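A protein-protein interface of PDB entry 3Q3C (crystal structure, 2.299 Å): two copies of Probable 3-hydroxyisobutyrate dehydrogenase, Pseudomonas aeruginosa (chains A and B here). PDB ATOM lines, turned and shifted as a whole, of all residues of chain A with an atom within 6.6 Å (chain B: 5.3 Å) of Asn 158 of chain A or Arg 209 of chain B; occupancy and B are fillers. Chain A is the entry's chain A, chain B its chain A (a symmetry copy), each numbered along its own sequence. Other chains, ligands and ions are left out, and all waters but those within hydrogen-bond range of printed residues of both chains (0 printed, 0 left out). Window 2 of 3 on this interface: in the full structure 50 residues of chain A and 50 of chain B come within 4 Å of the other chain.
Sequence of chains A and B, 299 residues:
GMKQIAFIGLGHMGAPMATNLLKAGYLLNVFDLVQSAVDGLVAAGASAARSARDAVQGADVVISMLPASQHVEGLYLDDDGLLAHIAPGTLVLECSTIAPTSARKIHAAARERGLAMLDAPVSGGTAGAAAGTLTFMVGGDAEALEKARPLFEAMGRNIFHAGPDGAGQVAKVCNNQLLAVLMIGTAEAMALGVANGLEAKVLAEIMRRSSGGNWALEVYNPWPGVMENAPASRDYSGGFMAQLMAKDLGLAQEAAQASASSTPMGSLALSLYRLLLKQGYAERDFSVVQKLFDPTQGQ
Hydrophobic or aromatic side chains of chain B within 4 Å of the printed part of chain A: Ile 206 and Met 207. Printed residues of chain A that touch a printed residue of chain B: Met 137, Asn 158, Phe 160, Asn 175 and Trp 215. Along chain A the printed residues that touch a printed residue of chain B span positions 137 to 215.
Met 137 of chain A touches Ile 206 of chain B. CE of Met 137 of chain A touches OG of Ser 210 of chain B, 3.9 Å away. Asn 158 of chain A touches Arg 209 of chain B (OD1 to NH1, 3.5 Å). Ile 206 of chain B touches Phe 160 of chain A. Phe 160 of chain A touches Arg 209 of chain B. CE of Met 207 of chain B touches CA of Asn 175 of chain A (3.1 Å). Ser 210 of chain B touches Asn 175 of chain A. CD1 of Trp 215 of chain A touches O of Ser 210 of chain B (3.5 Å). Ser 211 of chain B touches Trp 215 of chain A (O to CB, 3.1 Å).
The backbone NH (N) of Phe 136 of chain A is in hydrogen-bond range of the backbone carbonyl oxygen (O) of Asn 158 of chain A (3.0 Å). The backbone carbonyl oxygen (O) of Phe 136 of chain A sits at hydrogen-bond distance from the backbone NH (N) of Phe 160 of chain A (3.1 Å). OG of Ser 210 of chain B is in hydrogen-bond range of O of Ile 206 of chain B (2.8 Å).
ND2 of Asn 175 of chain A is in hydrogen-bond range of OG of Ser 211 of chain B (3.0 Å).
No position is printed for both chains.
Printed residues of chain B within 4 Å of Asn 158 of chain A: Arg 209. Ile 159 of chain A touches none of the printed residues of chain B. Printed residues of chain B within 4 Å of Phe 160 of chain A: Ile 206 (3.7 Å) and Arg 209 (3.8 Å). Of the printed residues of chain B, Asn 175 of chain A touches Met 207 (3.1 Å), Ser 210 (3.3 Å) and Ser 211 (3.0 Å). Of the printed residues of chain A, Met 207 of chain B touches Asn 175 (3.1 Å). Of the printed residues of chain A, Arg 209 of chain B touches Asn 158 and Phe 160. Printed residues of chain A within 4 Å of Ser 210 of chain B: Met 137 (3.9 Å), Asn 175 (3.3 Å) and Trp 215 (3.5 Å). The nearest printed residue of chain A that does not touch Arg 209 of chain B is Thr 135 of chain A (5.5 Å). The nearest printed residue of chain A that does not touch Ser 211 of chain B is Met 137 of chain A (6.0 Å).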
ATOM      1  N   THR A 133      20.920  -3.943  -1.216  1.00  0.00           N
ATOM      2  CA  THR A 133      19.586  -4.534  -1.264  1.00  0.00           C
ATOM      3  C   THR A 133      19.577  -6.067  -1.147  1.00  0.00           C
ATOM      4  O   THR A 133      18.540  -6.710  -1.364  1.00  0.00           O
ATOM      5  CB  THR A 133      18.898  -4.160  -2.579  1.00  0.00           C
ATOM      6  OG1 THR A 133      19.500  -4.888  -3.664  1.00  0.00           O
ATOM      7  CG2 THR A 133      19.038  -2.669  -2.829  1.00  0.00           C
ATOM      8  N   LEU A 134      20.726  -6.643  -0.806  1.00  0.00           N
ATOM      9  CA  LEU A 134      20.886  -8.094  -0.748  1.00  0.00           C
ATOM     10  C   LEU A 134      19.909  -8.764   0.201  1.00  0.00           C
ATOM     11  O   LEU A 134      19.401  -8.136   1.122  1.00  0.00           O
ATOM     12  CB  LEU A 134      22.300  -8.454  -0.311  1.00  0.00           C
ATOM     13  CG  LEU A 134      23.416  -8.024  -1.253  1.00  0.00           C
ATOM     14  CD1 LEU A 134      24.765  -8.341  -0.633  1.00  0.00           C
ATOM     15  CD2 LEU A 134      23.257  -8.686  -2.627  1.00  0.00           C
ATOM     16  N   THR A 135      19.664 -10.049  -0.034  1.00  0.00           N
ATOM     17  CA  THR A 135      18.872 -10.880   0.863  1.00  0.00           C
ATOM     18  C   THR A 135      19.784 -11.798   1.657  1.00  0.00           C
ATOM     19  O   THR A 135      20.603 -12.511   1.072  1.00  0.00           O
ATOM     20  CB  THR A 135      17.922 -11.776   0.079  1.00  0.00           C
ATOM     21  OG1 THR A 135      17.004 -10.960  -0.644  1.00  0.00           O
ATOM     22  CG2 THR A 135      17.158 -12.689   1.017  1.00  0.00           C
ATOM     23  N   PHE A 136      19.649 -11.780   2.982  1.00  0.00           N
ATOM     24  CA  PHE A 136      20.389 -12.718   3.805  1.00  0.00           C
ATOM     25  C   PHE A 136      19.491 -13.852   4.284  1.00  0.00           C
ATOM     26  O   PHE A 136      18.329 -13.634   4.635  1.00  0.00           O
ATOM     27  CB  PHE A 136      21.016 -12.034   5.011  1.00  0.00           C
ATOM     28  CG  PHE A 136      22.050 -11.026   4.671  1.00  0.00           C
ATOM     29  CD1 PHE A 136      23.390 -11.388   4.598  1.00  0.00           C
ATOM     30  CD2 PHE A 136      21.697  -9.699   4.456  1.00  0.00           C
ATOM     31  CE1 PHE A 136      24.371 -10.434   4.309  1.00  0.00           C
ATOM     32  CE2 PHE A 136      22.648  -8.757   4.147  1.00  0.00           C
ATOM     33  CZ  PHE A 136      23.999  -9.120   4.075  1.00  0.00           C
ATOM     34  N   MET A 137      20.054 -15.059   4.305  1.00  0.00           N
ATOM     35  CA  MET A 137      19.379 -16.249   4.816  1.00  0.00           C
ATOM     36  C   MET A 137      20.228 -16.823   5.939  1.00  0.00           C
ATOM     37  O   MET A 137      21.328 -17.318   5.707  1.00  0.00           O
ATOM     38  CB  MET A 137      19.191 -17.289   3.703  1.00  0.00           C
ATOM     39  CG  MET A 137      18.435 -16.737   2.513  1.00  0.00           C
ATOM     40  SD  MET A 137      18.361 -17.960   1.014  1.00  0.00           S
ATOM     41  CE  MET A 137      17.671 -16.730  -0.332  1.00  0.00           C
ATOM     42  N   PHE A 152      23.397  -6.271   8.759  1.00  0.00           N
ATOM     43  CA  PHE A 152      22.638  -6.836   7.653  1.00  0.00           C
ATOM     44  C   PHE A 152      21.817  -5.762   6.959  1.00  0.00           C
ATOM     45  O   PHE A 152      21.701  -5.753   5.733  1.00  0.00           O
ATOM     46  CB  PHE A 152      21.701  -7.947   8.140  1.00  0.00           C
ATOM     47  CG  PHE A 152      22.401  -9.231   8.501  1.00  0.00           C
ATOM     48  CD1 PHE A 152      21.934 -10.019   9.544  1.00  0.00           C
ATOM     49  CD2 PHE A 152      23.515  -9.657   7.797  1.00  0.00           C
ATOM     50  CE1 PHE A 152      22.562 -11.201   9.884  1.00  0.00           C
ATOM     51  CE2 PHE A 152      24.154 -10.840   8.132  1.00  0.00           C
ATOM     52  CZ  PHE A 152      23.671 -11.613   9.180  1.00  0.00           C
ATOM     53  N   GLY A 156      22.019  -5.000   3.278  1.00  0.00           N
ATOM     54  CA  GLY A 156      20.859  -5.594   2.647  1.00  0.00           C
ATOM     55  C   GLY A 156      19.473  -5.128   3.057  1.00  0.00           C
ATOM     56  O   GLY A 156      19.306  -4.173   3.817  1.00  0.00           O
ATOM     57  N   ARG A 157      18.473  -5.834   2.530  1.00  0.00           N
ATOM     58  CA  ARG A 157      17.069  -5.521   2.730  1.00  0.00           C
ATOM     59  C   ARG A 157      16.352  -6.692   3.413  1.00  0.00           C
ATOM     60  O   ARG A 157      16.220  -6.704   4.629  1.00  0.00           O
ATOM     61  CB  ARG A 157      16.426  -5.181   1.389  1.00  0.00           C
ATOM     62  CG  ARG A 157      14.997  -4.703   1.466  1.00  0.00           C
ATOM     63  CD  ARG A 157      14.530  -4.161   0.117  1.00  0.00           C
ATOM     64  NE  ARG A 157      14.944  -2.773  -0.084  1.00  0.00           N
ATOM     65  CZ  ARG A 157      14.856  -2.122  -1.239  1.00  0.00           C
ATOM     66  NH1 ARG A 157      14.374  -2.739  -2.314  1.00  0.00           N
ATOM     67  NH2 ARG A 157      15.260  -0.858  -1.322  1.00  0.00           N
ATOM     68  N   ASN A 158      15.897  -7.682   2.657  1.00  0.00           N
ATOM     69  CA  ASN A 158      15.263  -8.832   3.299  1.00  0.00           C
ATOM     70  C   ASN A 158      16.242  -9.631   4.152  1.00  0.00           C
ATOM     71  O   ASN A 158      17.291 -10.084   3.680  1.00  0.00           O
ATOM     72  CB  ASN A 158      14.574  -9.763   2.293  1.00  0.00           C
ATOM     73  CG  ASN A 158      13.414  -9.101   1.585  1.00  0.00           C
ATOM     74  OD1 ASN A 158      12.915  -8.063   2.026  1.00  0.00           O
ATOM     75  ND2 ASN A 158      12.987  -9.691   0.466  1.00  0.00           N
ATOM     76  N   ILE A 159      15.876  -9.798   5.414  1.00  0.00           N
ATOM     77  CA  ILE A 159      16.642 -10.599   6.347  1.00  0.00           C
ATOM     78  C   ILE A 159      15.705 -11.690   6.845  1.00  0.00           C
ATOM     79  O   ILE A 159      14.752 -11.420   7.581  1.00  0.00           O
ATOM     80  CB  ILE A 159      17.178  -9.738   7.519  1.00  0.00           C
ATOM     81  CG1 ILE A 159      17.870  -8.486   6.988  1.00  0.00           C
ATOM     82  CG2 ILE A 159      18.142 -10.526   8.380  1.00  0.00           C
ATOM     83  CD1 ILE A 159      18.281  -7.491   8.068  1.00  0.00           C
ATOM     84  N   PHE A 160      15.940 -12.919   6.398  1.00  0.00           N
ATOM     85  CA  PHE A 160      15.149 -14.051   6.868  1.00  0.00           C
ATOM     86  C   PHE A 160      15.945 -14.884   7.875  1.00  0.00           C
ATOM     87  O   PHE A 160      17.115 -15.195   7.652  1.00  0.00           O
ATOM     88  CB  PHE A 160      14.667 -14.936   5.698  1.00  0.00           C
ATOM     89  CG  PHE A 160      13.834 -14.202   4.668  1.00  0.00           C
ATOM     90  CD1 PHE A 160      14.427 -13.621   3.551  1.00  0.00           C
ATOM     91  CD2 PHE A 160      12.453 -14.120   4.799  1.00  0.00           C
ATOM     92  CE1 PHE A 160      13.662 -12.958   2.597  1.00  0.00           C
ATOM     93  CE2 PHE A 160      11.677 -13.454   3.841  1.00  0.00           C
ATOM     94  CZ  PHE A 160      12.286 -12.872   2.744  1.00  0.00           C
ATOM     95  N   ASN A 175      17.079 -22.593  -2.540  1.00  0.00           N
ATOM     96  CA  ASN A 175      16.564 -21.521  -3.372  1.00  0.00           C
ATOM     97  C   ASN A 175      17.237 -21.477  -4.743  1.00  0.00           C
ATOM     98  O   ASN A 175      16.567 -21.335  -5.764  1.00  0.00           O
ATOM     99  CB  ASN A 175      16.692 -20.178  -2.656  1.00  0.00           C
ATOM    100  CG  ASN A 175      16.391 -18.997  -3.558  1.00  0.00           C
ATOM    101  OD1 ASN A 175      15.232 -18.574  -3.713  1.00  0.00           O
ATOM    102  ND2 ASN A 175      17.440 -18.440  -4.148  1.00  0.00           N
ATOM    103  N   TRP A 215      10.251 -16.011 -11.139  1.00  0.00           N
ATOM    104  CA  TRP A 215      11.246 -14.980 -10.963  1.00  0.00           C
ATOM    105  C   TRP A 215      11.922 -14.590 -12.263  1.00  0.00           C
ATOM    106  O   TRP A 215      12.002 -13.397 -12.589  1.00  0.00           O
ATOM    107  CB  TRP A 215      12.307 -15.477 -10.013  1.00  0.00           C
ATOM    108  CG  TRP A 215      13.267 -14.448  -9.650  1.00  0.00           C
ATOM    109  CD1 TRP A 215      13.093 -13.468  -8.730  1.00  0.00           C
ATOM    110  CD2 TRP A 215      14.582 -14.272 -10.192  1.00  0.00           C
ATOM    111  NE1 TRP A 215      14.223 -12.695  -8.651  1.00  0.00           N
ATOM    112  CE2 TRP A 215      15.154 -13.167  -9.537  1.00  0.00           C
ATOM    113  CE3 TRP A 215      15.332 -14.946 -11.161  1.00  0.00           C
ATOM    114  CZ2 TRP A 215      16.442 -12.715  -9.820  1.00  0.00           C
ATOM    115  CZ3 TRP A 215      16.609 -14.498 -11.442  1.00  0.00           C
ATOM    116  CH2 TRP A 215      17.155 -13.398 -10.773  1.00  0.00           C
ATOM    117  N   ALA B 204       9.336 -21.967   2.559  1.00  0.00           N
ATOM    118  CA  ALA B 204       8.480 -21.571   1.455  1.00  0.00           C
ATOM    119  C   ALA B 204       8.556 -20.068   1.238  1.00  0.00           C
ATOM    120  O   ALA B 204       8.793 -19.597   0.126  1.00  0.00           O
ATOM    121  CB  ALA B 204       7.050 -22.004   1.703  1.00  0.00           C
ATOM    122  N   GLU B 205       8.360 -19.320   2.315  1.00  0.00           N
ATOM    123  CA  GLU B 205       8.316 -17.865   2.244  1.00  0.00           C
ATOM    124  C   GLU B 205       9.628 -17.280   1.731  1.00  0.00           C
ATOM    125  O   GLU B 205       9.650 -16.317   0.966  1.00  0.00           O
ATOM    126  CB  GLU B 205       7.976 -17.278   3.618  1.00  0.00           C
ATOM    127  CG  GLU B 205       7.403 -15.869   3.561  1.00  0.00           C
ATOM    128  CD  GLU B 205       6.169 -15.760   2.674  1.00  0.00           C
ATOM    129  OE1 GLU B 205       5.542 -16.796   2.372  1.00  0.00           O
ATOM    130  OE2 GLU B 205       5.827 -14.631   2.276  1.00  0.00           O
ATOM    131  N   ILE B 206      10.724 -17.871   2.167  1.00  0.00           N
ATOM    132  CA  ILE B 206      12.026 -17.461   1.698  1.00  0.00           C
ATOM    133  C   ILE B 206      12.128 -17.581   0.179  1.00  0.00           C
ATOM    134  O   ILE B 206      12.467 -16.619  -0.512  1.00  0.00           O
ATOM    135  CB  ILE B 206      13.124 -18.285   2.380  1.00  0.00           C
ATOM    136  CG1 ILE B 206      13.253 -17.852   3.849  1.00  0.00           C
ATOM    137  CG2 ILE B 206      14.436 -18.123   1.651  1.00  0.00           C
ATOM    138  CD1 ILE B 206      14.370 -18.554   4.617  1.00  0.00           C
ATOM    139  N   MET B 207      11.815 -18.756  -0.352  1.00  0.00           N
ATOM    140  CA  MET B 207      11.984 -18.951  -1.781  1.00  0.00           C
ATOM    141  C   MET B 207      10.987 -18.119  -2.576  1.00  0.00           C
ATOM    142  O   MET B 207      11.310 -17.637  -3.670  1.00  0.00           O
ATOM    143  CB  MET B 207      11.909 -20.429  -2.131  1.00  0.00           C
ATOM    144  CG  MET B 207      13.012 -21.232  -1.471  1.00  0.00           C
ATOM    145  SD  MET B 207      13.116 -23.028  -2.199  1.00  0.00           S
ATOM    146  CE  MET B 207      13.697 -22.543  -3.973  1.00  0.00           C
ATOM    147  N   ARG B 208       9.791 -17.942  -2.016  1.00  0.00           N
ATOM    148  CA  ARG B 208       8.739 -17.161  -2.663  1.00  0.00           C
ATOM    149  C   ARG B 208       9.202 -15.735  -2.879  1.00  0.00           C
ATOM    150  O   ARG B 208       9.038 -15.188  -3.949  1.00  0.00           O
ATOM    151  CB  ARG B 208       7.451 -17.139  -1.822  1.00  0.00           C
ATOM    152  CG  ARG B 208       6.244 -16.476  -2.530  1.00  0.00           C
ATOM    153  CD  ARG B 208       5.012 -16.273  -1.615  1.00  0.00           C
ATOM    154  NE  ARG B 208       5.245 -15.246  -0.591  1.00  0.00           N
ATOM    155  CZ  ARG B 208       5.144 -13.926  -0.793  1.00  0.00           C
ATOM    156  NH1 ARG B 208       4.784 -13.427  -1.979  1.00  0.00           N
ATOM    157  NH2 ARG B 208       5.412 -13.091   0.203  1.00  0.00           N
ATOM    158  N   ARG B 209       9.794 -15.140  -1.847  1.00  0.00           N
ATOM    159  CA  ARG B 209      10.231 -13.740  -1.897  1.00  0.00           C
ATOM    160  C   ARG B 209      11.592 -13.581  -2.590  1.00  0.00           C
ATOM    161  O   ARG B 209      12.124 -12.472  -2.701  1.00  0.00           O
ATOM    162  CB  ARG B 209      10.318 -13.157  -0.481  1.00  0.00           C
ATOM    163  CG  ARG B 209       9.006 -13.106   0.301  1.00  0.00           C
ATOM    164  CD  ARG B 209       8.772 -11.691   0.846  1.00  0.00           C
ATOM    165  NE  ARG B 209       8.713 -11.607   2.304  1.00  0.00           N
ATOM    166  CZ  ARG B 209       9.151 -10.561   3.003  1.00  0.00           C
ATOM    167  NH1 ARG B 209       9.711  -9.525   2.382  1.00  0.00           N
ATOM    168  NH2 ARG B 209       9.052 -10.553   4.328  1.00  0.00           N
ATOM    169  N   SER B 210      12.149 -14.689  -3.058  1.00  0.00           N
ATOM    170  CA  SER B 210      13.507 -14.688  -3.568  1.00  0.00           C
ATOM    171  C   SER B 210      13.657 -15.140  -5.022  1.00  0.00           C
ATOM    172  O   SER B 210      12.679 -15.251  -5.756  1.00  0.00           O
ATOM    173  CB  SER B 210      14.386 -15.519  -2.658  1.00  0.00           C
ATOM    174  OG  SER B 210      14.437 -14.887  -1.392  1.00  0.00           O
ATOM    175  N   SER B 211      14.892 -15.384  -5.440  1.00  0.00           N
ATOM    176  CA  SER B 211      15.114 -15.694  -6.840  1.00  0.00           C
ATOM    177  C   SER B 211      14.487 -17.058  -7.228  1.00  0.00           C
ATOM    178  O   SER B 211      14.237 -17.312  -8.386  1.00  0.00           O
ATOM    179  CB  SER B 211      16.607 -15.586  -7.212  1.00  0.00           C
ATOM    180  OG  SER B 211      17.404 -16.513  -6.486  1.00  0.00           O
